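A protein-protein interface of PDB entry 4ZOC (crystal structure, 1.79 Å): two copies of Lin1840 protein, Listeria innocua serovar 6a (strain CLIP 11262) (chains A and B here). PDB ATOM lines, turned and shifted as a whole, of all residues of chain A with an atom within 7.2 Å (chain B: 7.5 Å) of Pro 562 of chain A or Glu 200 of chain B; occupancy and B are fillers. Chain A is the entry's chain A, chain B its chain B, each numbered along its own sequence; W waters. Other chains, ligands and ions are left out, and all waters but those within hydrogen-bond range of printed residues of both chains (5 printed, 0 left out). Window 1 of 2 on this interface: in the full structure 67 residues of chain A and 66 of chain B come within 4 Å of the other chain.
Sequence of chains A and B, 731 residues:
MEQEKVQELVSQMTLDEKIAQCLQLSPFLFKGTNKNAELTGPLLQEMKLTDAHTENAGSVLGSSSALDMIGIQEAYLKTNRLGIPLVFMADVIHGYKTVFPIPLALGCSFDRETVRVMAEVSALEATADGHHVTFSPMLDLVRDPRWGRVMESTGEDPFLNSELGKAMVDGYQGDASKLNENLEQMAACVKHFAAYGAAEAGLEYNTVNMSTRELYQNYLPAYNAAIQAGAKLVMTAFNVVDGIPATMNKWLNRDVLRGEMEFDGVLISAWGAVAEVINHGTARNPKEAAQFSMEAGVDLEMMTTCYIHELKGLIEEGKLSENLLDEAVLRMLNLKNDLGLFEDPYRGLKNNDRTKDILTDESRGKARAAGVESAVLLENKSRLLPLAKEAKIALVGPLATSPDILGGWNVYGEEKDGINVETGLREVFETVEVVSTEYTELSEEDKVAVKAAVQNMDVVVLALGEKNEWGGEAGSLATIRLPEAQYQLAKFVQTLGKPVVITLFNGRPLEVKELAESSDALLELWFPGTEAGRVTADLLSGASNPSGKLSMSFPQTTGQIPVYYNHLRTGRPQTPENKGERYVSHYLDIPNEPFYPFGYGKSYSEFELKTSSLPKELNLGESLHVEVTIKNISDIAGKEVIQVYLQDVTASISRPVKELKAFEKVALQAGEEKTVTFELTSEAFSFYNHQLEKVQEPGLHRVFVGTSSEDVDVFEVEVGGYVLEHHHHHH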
ATOM      1  N   ARG A 143      23.470 -15.383  15.567  1.00  0.00           N
ATOM      2  CA  ARG A 143      24.535 -16.371  15.364  1.00  0.00           C
ATOM      3  C   ARG A 143      23.983 -17.702  14.784  1.00  0.00           C
ATOM      4  O   ARG A 143      24.754 -18.657  14.683  1.00  0.00           O
ATOM      5  CB  ARG A 143      25.218 -16.648  16.659  1.00  0.00           C
ATOM      6  CG  ARG A 143      25.995 -15.495  17.214  1.00  0.00           C
ATOM      7  CD  ARG A 143      26.444 -15.838  18.632  1.00  0.00           C
ATOM      8  NE  ARG A 143      27.341 -14.797  19.138  1.00  0.00           N
ATOM      9  CZ  ARG A 143      27.866 -14.780  20.360  1.00  0.00           C
ATOM     10  NH1 ARG A 143      27.599 -15.746  21.198  1.00  0.00           N
ATOM     11  NH2 ARG A 143      28.667 -13.787  20.737  1.00  0.00           N
ATOM     12  N   ASP A 144      22.688 -17.755  14.436  1.00  0.00           N
ATOM     13  CA  ASP A 144      22.001 -19.013  14.131  1.00  0.00           C
ATOM     14  C   ASP A 144      21.135 -18.813  12.901  1.00  0.00           C
ATOM     15  O   ASP A 144      20.008 -18.348  12.953  1.00  0.00           O
ATOM     16  CB  ASP A 144      21.198 -19.503  15.347  1.00  0.00           C
ATOM     17  CG  ASP A 144      20.632 -20.893  15.146  1.00  0.00           C
ATOM     18  OD1 ASP A 144      20.574 -21.376  13.952  1.00  0.00           O
ATOM     19  OD2 ASP A 144      20.212 -21.493  16.176  1.00  0.00           O
ATOM     20  N   PRO A 145      21.673 -19.176  11.731  1.00  0.00           N
ATOM     21  CA  PRO A 145      20.944 -19.008  10.518  1.00  0.00           C
ATOM     22  C   PRO A 145      19.755 -19.937  10.286  1.00  0.00           C
ATOM     23  O   PRO A 145      19.052 -19.783   9.262  1.00  0.00           O
ATOM     24  CB  PRO A 145      22.015 -19.182   9.456  1.00  0.00           C
ATOM     25  CG  PRO A 145      23.058 -19.987  10.059  1.00  0.00           C
ATOM     26  CD  PRO A 145      23.023 -19.728  11.545  1.00  0.00           C
ATOM     27  N   ARG A 146      19.463 -20.863  11.220  1.00  0.00           N
ATOM     28  CA  ARG A 146      18.164 -21.632  11.145  1.00  0.00           C
ATOM     29  C   ARG A 146      17.030 -20.675  11.320  1.00  0.00           C
ATOM     30  O   ARG A 146      15.951 -20.835  10.701  1.00  0.00           O
ATOM     31  CB  ARG A 146      18.119 -22.705  12.220  1.00  0.00           C
ATOM     32  CG  ARG A 146      19.049 -23.839  11.918  1.00  0.00           C
ATOM     33  CD  ARG A 146      19.182 -24.782  13.090  1.00  0.00           C
ATOM     34  NE  ARG A 146      19.845 -24.160  14.233  1.00  0.00           N
ATOM     35  CZ  ARG A 146      20.254 -24.829  15.309  1.00  0.00           C
ATOM     36  NH1 ARG A 146      20.037 -26.117  15.432  1.00  0.00           N
ATOM     37  NH2 ARG A 146      20.892 -24.191  16.283  1.00  0.00           N
ATOM     38  N   TYR A 219      24.659  -8.672  23.478  1.00  0.00           N
ATOM     39  CA  TYR A 219      23.256  -8.674  23.010  1.00  0.00           C
ATOM     40  C   TYR A 219      22.576  -7.317  23.179  1.00  0.00           C
ATOM     41  O   TYR A 219      21.640  -7.015  22.438  1.00  0.00           O
ATOM     42  CB  TYR A 219      22.462  -9.780  23.735  1.00  0.00           C
ATOM     43  CG  TYR A 219      22.800 -11.091  23.137  1.00  0.00           C
ATOM     44  CD1 TYR A 219      23.920 -11.752  23.522  1.00  0.00           C
ATOM     45  CD2 TYR A 219      22.039 -11.637  22.073  1.00  0.00           C
ATOM     46  CE1 TYR A 219      24.292 -12.915  22.898  1.00  0.00           C
ATOM     47  CE2 TYR A 219      22.399 -12.818  21.511  1.00  0.00           C
ATOM     48  CZ  TYR A 219      23.524 -13.461  21.941  1.00  0.00           C
ATOM     49  OH  TYR A 219      23.939 -14.617  21.283  1.00  0.00           O
ATOM     50  N   PRO A 555      28.136 -21.400   7.582  1.00  0.00           N
ATOM     51  CA  PRO A 555      28.652 -22.645   8.105  1.00  0.00           C
ATOM     52  C   PRO A 555      29.047 -23.675   7.088  1.00  0.00           C
ATOM     53  O   PRO A 555      28.543 -23.767   5.971  1.00  0.00           O
ATOM     54  CB  PRO A 555      27.529 -23.159   9.011  1.00  0.00           C
ATOM     55  CG  PRO A 555      26.659 -21.950   9.302  1.00  0.00           C
ATOM     56  CD  PRO A 555      26.764 -21.186   8.011  1.00  0.00           C
ATOM     57  N   THR A 558      25.020 -27.547   8.861  1.00  0.00           N
ATOM     58  CA  THR A 558      24.044 -27.126   9.865  1.00  0.00           C
ATOM     59  C   THR A 558      24.573 -27.365  11.290  1.00  0.00           C
ATOM     60  O   THR A 558      24.425 -26.534  12.183  1.00  0.00           O
ATOM     61  CB  THR A 558      22.692 -27.907   9.622  1.00  0.00           C
ATOM     62  OG1 THR A 558      22.120 -27.412   8.381  1.00  0.00           O
ATOM     63  CG2 THR A 558      21.754 -27.655  10.714  1.00  0.00           C
ATOM     64  N   GLY A 559      25.179 -28.531  11.492  1.00  0.00           N
ATOM     65  CA  GLY A 559      25.682 -28.891  12.800  1.00  0.00           C
ATOM     66  C   GLY A 559      26.906 -28.139  13.305  1.00  0.00           C
ATOM     67  O   GLY A 559      27.266 -28.328  14.467  1.00  0.00           O
ATOM     68  N   GLN A 560      27.490 -27.273  12.524  1.00  0.00           N
ATOM     69  CA  GLN A 560      28.518 -26.361  12.997  1.00  0.00           C
ATOM     70  C   GLN A 560      27.921 -25.173  13.799  1.00  0.00           C
ATOM     71  O   GLN A 560      28.619 -24.410  14.447  1.00  0.00           O
ATOM     72  CB  GLN A 560      29.326 -25.848  11.809  1.00  0.00           C
ATOM     73  CG  GLN A 560      30.690 -25.276  12.259  1.00  0.00           C
ATOM     74  CD  GLN A 560      31.525 -24.719  11.104  1.00  0.00           C
ATOM     75  OE1 GLN A 560      31.005 -24.070  10.177  1.00  0.00           O
ATOM     76  NE2 GLN A 560      32.812 -25.082  11.085  1.00  0.00           N
ATOM     77  N   ILE A 561      26.629 -24.961  13.678  1.00  0.00           N
ATOM     78  CA  ILE A 561      25.947 -23.820  14.317  1.00  0.00           C
ATOM     79  C   ILE A 561      25.913 -23.915  15.863  1.00  0.00           C
ATOM     80  O   ILE A 561      25.548 -24.972  16.409  1.00  0.00           O
ATOM     81  CB  ILE A 561      24.532 -23.681  13.758  1.00  0.00           C
ATOM     82  CG1 ILE A 561      24.569 -23.320  12.270  1.00  0.00           C
ATOM     83  CG2 ILE A 561      23.785 -22.606  14.547  1.00  0.00           C
ATOM     84  CD1 ILE A 561      23.194 -23.408  11.622  1.00  0.00           C
ATOM     85  N   PRO A 562      26.268 -22.837  16.575  1.00  0.00           N
ATOM     86  CA  PRO A 562      26.661 -21.543  16.024  1.00  0.00           C
ATOM     87  C   PRO A 562      28.147 -21.422  15.821  1.00  0.00           C
ATOM     88  O   PRO A 562      28.952 -21.930  16.672  1.00  0.00           O
ATOM     89  CB  PRO A 562      26.318 -20.565  17.149  1.00  0.00           C
ATOM     90  CG  PRO A 562      26.457 -21.362  18.414  1.00  0.00           C
ATOM     91  CD  PRO A 562      25.893 -22.705  18.015  1.00  0.00           C
ATOM     92  N   VAL A 563      28.492 -20.786  14.715  1.00  0.00           N
ATOM     93  CA  VAL A 563      29.867 -20.520  14.357  1.00  0.00           C
ATOM     94  C   VAL A 563      29.964 -19.013  14.024  1.00  0.00           C
ATOM     95  O   VAL A 563      29.141 -18.471  13.255  1.00  0.00           O
ATOM     96  CB  VAL A 563      30.352 -21.408  13.172  1.00  0.00           C
ATOM     97  CG1 VAL A 563      29.509 -21.252  11.921  1.00  0.00           C
ATOM     98  CG2 VAL A 563      31.808 -21.101  12.906  1.00  0.00           C
ATOM     99  N   TYR A 564      30.972 -18.336  14.578  1.00  0.00           N
ATOM    100  CA  TYR A 564      31.046 -16.903  14.449  1.00  0.00           C
ATOM    101  C   TYR A 564      32.479 -16.446  14.687  1.00  0.00           C
ATOM    102  O   TYR A 564      33.252 -17.187  15.359  1.00  0.00           O
ATOM    103  CB  TYR A 564      29.992 -16.244  15.395  1.00  0.00           C
ATOM    104  CG  TYR A 564      30.032 -16.719  16.814  1.00  0.00           C
ATOM    105  CD1 TYR A 564      30.864 -16.111  17.732  1.00  0.00           C
ATOM    106  CD2 TYR A 564      29.315 -17.816  17.242  1.00  0.00           C
ATOM    107  CE1 TYR A 564      30.916 -16.517  19.058  1.00  0.00           C
ATOM    108  CE2 TYR A 564      29.381 -18.252  18.565  1.00  0.00           C
ATOM    109  CZ  TYR A 564      30.149 -17.602  19.476  1.00  0.00           C
ATOM    110  OH  TYR A 564      30.242 -18.064  20.727  1.00  0.00           O
ATOM    111  N   HIS A 567      34.727 -15.462  18.584  1.00  0.00           N
ATOM    112  CA  HIS A 567      34.641 -16.587  19.465  1.00  0.00           C
ATOM    113  C   HIS A 567      35.782 -16.628  20.501  1.00  0.00           C
ATOM    114  O   HIS A 567      36.793 -15.997  20.315  1.00  0.00           O
ATOM    115  CB  HIS A 567      34.599 -17.902  18.660  1.00  0.00           C
ATOM    116  CG  HIS A 567      35.840 -18.157  17.900  1.00  0.00           C
ATOM    117  ND1 HIS A 567      36.970 -18.712  18.474  1.00  0.00           N
ATOM    118  CD2 HIS A 567      36.166 -17.896  16.613  1.00  0.00           C
ATOM    119  CE1 HIS A 567      37.930 -18.794  17.567  1.00  0.00           C
ATOM    120  NE2 HIS A 567      37.473 -18.300  16.443  1.00  0.00           N
ATOM    121  N   LEU A 568      35.526 -17.333  21.607  1.00  0.00           N
ATOM    122  CA  LEU A 568      36.530 -17.585  22.612  1.00  0.00           C
ATOM    123  C   LEU A 568      37.547 -18.627  22.195  1.00  0.00           C
ATOM    124  O   LEU A 568      37.337 -19.485  21.347  1.00  0.00           O
ATOM    125  CB  LEU A 568      35.902 -17.963  23.954  1.00  0.00           C
ATOM    126  CG  LEU A 568      34.788 -17.017  24.504  1.00  0.00           C
ATOM    127  CD1 LEU A 568      34.439 -17.458  25.914  1.00  0.00           C
ATOM    128  CD2 LEU A 568      35.199 -15.567  24.500  1.00  0.00           C
ATOM    129  N   TYR A 587      36.200 -30.817  15.425  1.00  0.00           N
ATOM    130  CA  TYR A 587      35.265 -31.832  15.044  1.00  0.00           C
ATOM    131  C   TYR A 587      35.978 -32.979  14.276  1.00  0.00           C
ATOM    132  O   TYR A 587      36.868 -32.774  13.470  1.00  0.00           O
ATOM    133  CB  TYR A 587      34.198 -31.324  14.094  1.00  0.00           C
ATOM    134  CG  TYR A 587      33.215 -30.315  14.685  1.00  0.00           C
ATOM    135  CD1 TYR A 587      32.110 -30.740  15.459  1.00  0.00           C
ATOM    136  CD2 TYR A 587      33.402 -28.950  14.464  1.00  0.00           C
ATOM    137  CE1 TYR A 587      31.229 -29.795  15.979  1.00  0.00           C
ATOM    138  CE2 TYR A 587      32.553 -28.010  14.987  1.00  0.00           C
ATOM    139  CZ  TYR A 587      31.442 -28.448  15.724  1.00  0.00           C
ATOM    140  OH  TYR A 587      30.588 -27.495  16.221  1.00  0.00           O
ATOM    141  N   ASP B 144      23.030 -32.196  23.881  1.00  0.00           N
ATOM    142  CA  ASP B 144      23.645 -31.974  22.579  1.00  0.00           C
ATOM    143  C   ASP B 144      24.446 -33.216  22.209  1.00  0.00           C
ATOM    144  O   ASP B 144      25.559 -33.397  22.632  1.00  0.00           O
ATOM    145  CB  ASP B 144      24.502 -30.687  22.569  1.00  0.00           C
ATOM    146  CG  ASP B 144      24.975 -30.316  21.181  1.00  0.00           C
ATOM    147  OD1 ASP B 144      24.956 -31.192  20.285  1.00  0.00           O
ATOM    148  OD2 ASP B 144      25.434 -29.176  20.986  1.00  0.00           O
ATOM    149  N   ARG B 146      25.896 -34.048  19.574  1.00  0.00           N
ATOM    150  CA  ARG B 146      27.110 -33.836  18.792  1.00  0.00           C
ATOM    151  C   ARG B 146      28.335 -34.086  19.672  1.00  0.00           C
ATOM    152  O   ARG B 146      29.366 -34.594  19.197  1.00  0.00           O
ATOM    153  CB  ARG B 146      27.214 -32.397  18.183  1.00  0.00           C
ATOM    154  CG  ARG B 146      26.204 -32.186  17.118  1.00  0.00           C
ATOM    155  CD  ARG B 146      26.163 -30.742  16.715  1.00  0.00           C
ATOM    156  NE  ARG B 146      25.541 -29.924  17.716  1.00  0.00           N
ATOM    157  CZ  ARG B 146      25.211 -28.643  17.568  1.00  0.00           C
ATOM    158  NH1 ARG B 146      25.455 -27.965  16.437  1.00  0.00           N
ATOM    159  NH2 ARG B 146      24.642 -28.019  18.590  1.00  0.00           N
ATOM    160  N   TRP B 147      28.253 -33.721  20.931  1.00  0.00           N
ATOM    161  CA  TRP B 147      29.386 -33.839  21.893  1.00  0.00           C
ATOM    162  C   TRP B 147      29.646 -35.318  22.186  1.00  0.00           C
ATOM    163  O   TRP B 147      28.715 -36.064  22.588  1.00  0.00           O
ATOM    164  CB  TRP B 147      28.972 -33.164  23.207  1.00  0.00           C
ATOM    165  CG  TRP B 147      30.040 -32.883  24.166  1.00  0.00           C
ATOM    166  CD1 TRP B 147      31.239 -32.340  23.906  1.00  0.00           C
ATOM    167  CD2 TRP B 147      29.990 -33.130  25.573  1.00  0.00           C
ATOM    168  NE1 TRP B 147      31.911 -32.144  25.080  1.00  0.00           N
ATOM    169  CE2 TRP B 147      31.176 -32.608  26.112  1.00  0.00           C
ATOM    170  CE3 TRP B 147      29.024 -33.679  26.448  1.00  0.00           C
ATOM    171  CZ2 TRP B 147      31.459 -32.647  27.473  1.00  0.00           C
ATOM    172  CZ3 TRP B 147      29.336 -33.741  27.803  1.00  0.00           C
ATOM    173  CH2 TRP B 147      30.499 -33.177  28.284  1.00  0.00           C
ATOM    174  N   TYR B 196      29.938 -28.656  31.777  1.00  0.00           N
ATOM    175  CA  TYR B 196      30.826 -28.986  30.664  1.00  0.00           C
ATOM    176  C   TYR B 196      30.042 -29.481  29.436  1.00  0.00           C
ATOM    177  O   TYR B 196      30.460 -29.224  28.325  1.00  0.00           O
ATOM    178  CB  TYR B 196      31.871 -30.032  31.209  1.00  0.00           C
ATOM    179  CG  TYR B 196      32.897 -30.599  30.257  1.00  0.00           C
ATOM    180  CD1 TYR B 196      33.495 -29.852  29.266  1.00  0.00           C
ATOM    181  CD2 TYR B 196      33.384 -31.880  30.439  1.00  0.00           C
ATOM    182  CE1 TYR B 196      34.438 -30.375  28.379  1.00  0.00           C
ATOM    183  CE2 TYR B 196      34.343 -32.376  29.565  1.00  0.00           C
ATOM    184  CZ  TYR B 196      34.863 -31.668  28.568  1.00  0.00           C
ATOM    185  OH  TYR B 196      35.826 -32.278  27.785  1.00  0.00           O
ATOM    186  N   GLY B 197      28.918 -30.138  29.700  1.00  0.00           N
ATOM    187  CA  GLY B 197      28.045 -30.719  28.709  1.00  0.00           C
ATOM    188  C   GLY B 197      27.328 -29.741  27.816  1.00  0.00           C
ATOM    189  O   GLY B 197      26.770 -30.161  26.826  1.00  0.00           O
ATOM    190  N   ALA B 198      27.346 -28.446  28.176  1.00  0.00           N
ATOM    191  CA  ALA B 198      26.750 -27.387  27.379  1.00  0.00           C
ATOM    192  C   ALA B 198      27.667 -26.797  26.328  1.00  0.00           C
ATOM    193  O   ALA B 198      27.338 -25.783  25.762  1.00  0.00           O
ATOM    194  CB  ALA B 198      26.232 -26.308  28.279  1.00  0.00           C
ATOM    195  N   ALA B 199      28.759 -27.492  25.998  1.00  0.00           N
ATOM    196  CA  ALA B 199      29.751 -27.026  25.051  1.00  0.00           C
ATOM    197  C   ALA B 199      29.034 -26.604  23.786  1.00  0.00           C
ATOM    198  O   ALA B 199      28.228 -27.352  23.167  1.00  0.00           O
ATOM    199  CB  ALA B 199      30.684 -28.162  24.704  1.00  0.00           C
ATOM    200  N   GLU B 200      29.291 -25.366  23.430  1.00  0.00           N
ATOM    201  CA  GLU B 200      28.613 -24.773  22.289  1.00  0.00           C
ATOM    202  C   GLU B 200      28.905 -25.527  20.962  1.00  0.00           C
ATOM    203  O   GLU B 200      30.048 -25.919  20.687  1.00  0.00           O
ATOM    204  CB  GLU B 200      29.038 -23.315  22.166  1.00  0.00           C
ATOM    205  CG  GLU B 200      28.133 -22.419  21.373  1.00  0.00           C
ATOM    206  CD  GLU B 200      28.462 -20.957  21.611  1.00  0.00           C
ATOM    207  OE1 GLU B 200      29.409 -20.567  20.950  1.00  0.00           O
ATOM    208  OE2 GLU B 200      27.858 -20.284  22.508  1.00  0.00           O
ATOM    209  N   ALA B 201      27.841 -25.733  20.191  1.00  0.00           N
ATOM    210  CA  ALA B 201      27.854 -26.452  18.916  1.00  0.00           C
ATOM    211  C   ALA B 201      28.352 -27.893  19.011  1.00  0.00           C
ATOM    212  O   ALA B 201      28.812 -28.463  18.060  1.00  0.00           O
ATOM    213  CB  ALA B 201      28.634 -25.627  17.913  1.00  0.00           C
ATOM    214  N   GLY B 202      28.316 -28.455  20.221  1.00  0.00           N
ATOM    215  CA  GLY B 202      28.808 -29.794  20.455  1.00  0.00           C
ATOM    216  C   GLY B 202      30.287 -29.969  20.350  1.00  0.00           C
ATOM    217  O   GLY B 202      30.781 -31.070  20.375  1.00  0.00           O
ATOM    218  N   LEU B 203      31.019 -28.876  20.377  1.00  0.00           N
ATOM    219  CA  LEU B 203      32.431 -28.886  20.026  1.00  0.00           C
ATOM    220  C   LEU B 203      33.283 -29.053  21.262  1.00  0.00           C
ATOM    221  O   LEU B 203      33.074 -28.374  22.238  1.00  0.00           O
ATOM    222  CB  LEU B 203      32.782 -27.603  19.317  1.00  0.00           C
ATOM    223  CG  LEU B 203      34.212 -27.348  18.934  1.00  0.00           C
ATOM    224  CD1 LEU B 203      34.790 -28.435  18.042  1.00  0.00           C
ATOM    225  CD2 LEU B 203      34.376 -25.955  18.286  1.00  0.00           C
ATOM    226  N   GLU B 204      34.176 -30.011  21.244  1.00  0.00           N
ATOM    227  CA  GLU B 204      34.936 -30.351  22.441  1.00  0.00           C
ATOM    228  C   GLU B 204      35.671 -29.140  22.995  1.00  0.00           C
ATOM    229  O   GLU B 204      36.301 -28.343  22.284  1.00  0.00           O
ATOM    230  CB  GLU B 204      35.887 -31.524  22.201  1.00  0.00           C
ATOM    231  CG  GLU B 204      36.493 -32.023  23.515  1.00  0.00           C
ATOM    232  CD  GLU B 204      35.434 -32.575  24.394  1.00  0.00           C
ATOM    233  OE1 GLU B 204      34.949 -33.714  24.152  1.00  0.00           O
ATOM    234  OE2 GLU B 204      34.895 -31.878  25.298  1.00  0.00           O
ATOM    235  N   TYR B 205      35.528 -29.003  24.321  1.00  0.00           N
ATOM    236  CA  TYR B 205      36.220 -27.977  25.149  1.00  0.00           C
ATOM    237  C   TYR B 205      35.654 -26.599  24.899  1.00  0.00           C
ATOM    238  O   TYR B 205      36.207 -25.620  25.341  1.00  0.00           O
ATOM    239  CB  TYR B 205      37.753 -27.976  24.944  1.00  0.00           C
ATOM    240  CG  TYR B 205      38.437 -29.349  24.952  1.00  0.00           C
ATOM    241  CD1 TYR B 205      38.409 -30.160  26.055  1.00  0.00           C
ATOM    242  CD2 TYR B 205      39.110 -29.817  23.847  1.00  0.00           C
ATOM    243  CE1 TYR B 205      39.019 -31.437  26.070  1.00  0.00           C
ATOM    244  CE2 TYR B 205      39.712 -31.080  23.837  1.00  0.00           C
ATOM    245  CZ  TYR B 205      39.676 -31.881  24.980  1.00  0.00           C
ATOM    246  OH  TYR B 205      40.290 -33.123  24.938  1.00  0.00           O
ATOM    247  N   ASN B 206      34.576 -26.505  24.152  1.00  0.00           N
ATOM    248  CA  ASN B 206      34.200 -25.182  23.680  1.00  0.00           C
ATOM    249  C   ASN B 206      33.466 -24.405  24.808  1.00  0.00           C
ATOM    250  O   ASN B 206      33.026 -24.965  25.830  1.00  0.00           O
ATOM    251  CB  ASN B 206      33.305 -25.327  22.434  1.00  0.00           C
ATOM    252  CG  ASN B 206      33.219 -24.048  21.605  1.00  0.00           C
ATOM    253  OD1 ASN B 206      34.067 -23.114  21.699  1.00  0.00           O
ATOM    254  ND2 ASN B 206      32.202 -23.995  20.754  1.00  0.00           N
ATOM    255  N   THR B 207      33.249 -23.129  24.518  1.00  0.00           N
ATOM    256  CA  THR B 207      32.439 -22.243  25.304  1.00  0.00           C
ATOM    257  C   THR B 207      31.201 -22.804  25.855  1.00  0.00           C
ATOM    258  O   THR B 207      30.381 -23.468  25.182  1.00  0.00           O
ATOM    259  CB  THR B 207      32.164 -21.010  24.474  1.00  0.00           C
ATOM    260  OG1 THR B 207      33.398 -20.456  24.058  1.00  0.00           O
ATOM    261  CG2 THR B 207      31.303 -19.933  25.184  1.00  0.00           C
ATOM    262  N   VAL B 208      31.002 -22.505  27.112  1.00  0.00           N
ATOM    263  CA  VAL B 208      29.715 -22.771  27.802  1.00  0.00           C
ATOM    264  C   VAL B 208      29.174 -21.437  28.286  1.00  0.00           C
ATOM    265  O   VAL B 208      29.929 -20.661  28.914  1.00  0.00           O
ATOM    266  CB  VAL B 208      29.911 -23.800  28.974  1.00  0.00           C
ATOM    267  CG1 VAL B 208      28.717 -23.882  29.917  1.00  0.00           C
ATOM    268  CG2 VAL B 208      30.245 -25.186  28.478  1.00  0.00           C
ATOM    269  N   ASN B 209      27.906 -21.163  28.049  1.00  0.00           N
ATOM    270  CA  ASN B 209      27.290 -19.980  28.660  1.00  0.00           C
ATOM    271  C   ASN B 209      25.827 -20.223  28.948  1.00  0.00           C
ATOM    272  O   ASN B 209      25.093 -20.683  28.080  1.00  0.00           O
ATOM    273  CB  ASN B 209      27.399 -18.773  27.740  1.00  0.00           C
ATOM    274  CG  ASN B 209      26.960 -17.497  28.399  1.00  0.00           C
ATOM    275  OD1 ASN B 209      25.838 -17.044  28.191  1.00  0.00           O
ATOM    276  ND2 ASN B 209      27.818 -16.947  29.270  1.00  0.00           N
ATOM    277  N   SER B 476      33.797 -35.114  18.715  1.00  0.00           N
ATOM    278  CA  SER B 476      32.635 -34.302  18.333  1.00  0.00           C
ATOM    279  C   SER B 476      32.269 -34.570  16.908  1.00  0.00           C
ATOM    280  O   SER B 476      33.170 -34.528  16.058  1.00  0.00           O
ATOM    281  CB  SER B 476      32.974 -32.821  18.501  1.00  0.00           C
ATOM    282  OG  SER B 476      33.077 -32.460  19.891  1.00  0.00           O
HETATM  283  O   HOH W   1      24.196 -25.327  18.543  1.00  0.00           O
HETATM  284  O   HOH W   2      32.986 -18.947  21.848  1.00  0.00           O
HETATM  285  O   HOH W   3      31.480 -22.713  17.778  1.00  0.00           O
HETATM  286  O   HOH W   4      26.448 -18.252  21.190  1.00  0.00           O
HETATM  287  O   HOH W   5      34.922 -20.859  20.446  1.00  0.00           O
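The backbone carbonyl oxygen (O) of Gly 559 of chain A sits at hydrogen-bond distance from the guanidinium group (NH1) of Arg 146 of chain B, at 2.7 Å.
The backbone carbonyl oxygen of Ile 561 of chain A sits at hydrogen-bond distance from the guanidinium group of Arg 146 of chain B.
The side-chain hydroxyl of Tyr 564 of chain A lies within hydrogen-bond range of the side-chain carboxylate of Glu 200 of chain B, 2.6 Å away.
The backbone carbonyl oxygen of Ala 201 of chain B is in hydrogen-bond range of the side-chain hydroxyl of Tyr 587 of chain A, 2.7 Å away.
The guanidinium group (NH2) of Arg 146 of chain B is in salt-bridge range of the side-chain carboxylate (OD2) of Asp 144 of chain B (2.8 Å).
The backbone carbonyl oxygen (O) of Glu 200 of chain B is in hydrogen-bond range of the side-chain amide nitrogen (ND2) of Asn 206 of chain B (2.9 Å).
O of Thr 207 of chain B sits at hydrogen-bond distance from N of Glu 200 of chain B (2.8 Å).
OG of Ser 476 of chain B lies within hydrogen-bond range of O of Gly 202 of chain B (2.7 Å).
N of Glu 204 of chain B sits at hydrogen-bond distance from OG of Ser 476 of chain B.
Among the printed residues, merely in contact across the chains: Gly 559 of chain A with Ala 201 of chain B, Gln 560 of chain A with Ala 201 of chain B, Ile 561 of chain A with Ala 201 of chain B, Pro 562 of chain A with Glu 200 of chain B, Pro 562 of chain A with Ala 201 of chain B, Leu 568 of chain A with Thr 207 of chain B, Tyr 587 of chain A with Leu 203 of chain B and Tyr 587 of chain A with Ser 476 of chain B.
Pro 562 of chain A touches just these residues of chain B: Glu 200 and Ala 201.
Of the printed residues of chain A, Glu 200 of chain B touches Pro 562 (3.6 Å) and Tyr 564 (2.6 Å).
Of the printed residues of chain A, Leu 203 of chain B touches Tyr 587.
Of the printed residues of chain B, Gln 560 of chain A touches Ala 201 (3.7 Å).
Of the printed residues of chain A, Arg 146 of chain B touches Gly 559 and Ile 561.
Printed residues of chain A within 4 Å of Ser 476 of chain B: Tyr 587 (3.6 Å).
The nearest residue of chain A that does not touch Glu 200 of chain B is Arg 143 of chain A (4.7 Å).
The nearest printed residue of chain A that does not touch Thr 207 of chain B is Tyr 564 of chain A (4.9 Å).
Of the 18 printed residues of chain B, 6 touch a printed residue of chain A.
Hydrophobic or aromatic side chains of chain A within 4 Å of the printed part of chain B: Pro 562, Tyr 564, Leu 568 and Tyr 587.
Positions printed for both chains: 144 and 146.
Of the 12 pairs that touch across the chains among the printed residues, none has its exchanged pair printed and touching as well.
Water W1 bridges O of Ile 561 of chain A (2.6 Å) and NH2 of Arg 146 of chain B (2.7 Å).
Water W2 lies within hydrogen-bond range of the side-chain hydroxyl of Thr 207 of chain B (2.7 Å), the backbone NH of Leu 568 of chain A (3.0 Å) and the side-chain hydroxyl of Tyr 564 of chain A (3.1 Å).
Water W5 bridges OD1 of Asn 206 of chain B (2.7 Å) and O of Leu 568 of chain A (2.9 Å).
Water W4 bridges the guanidinium group (NH1) of Arg 143 of chain A (2.8 Å) and the side-chain carboxylate (OE2) of Glu 200 of chain B (2.8 Å).
Water W3 bridges O of Pro 562 of chain A and ND2 of Asn 206 of chain B.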
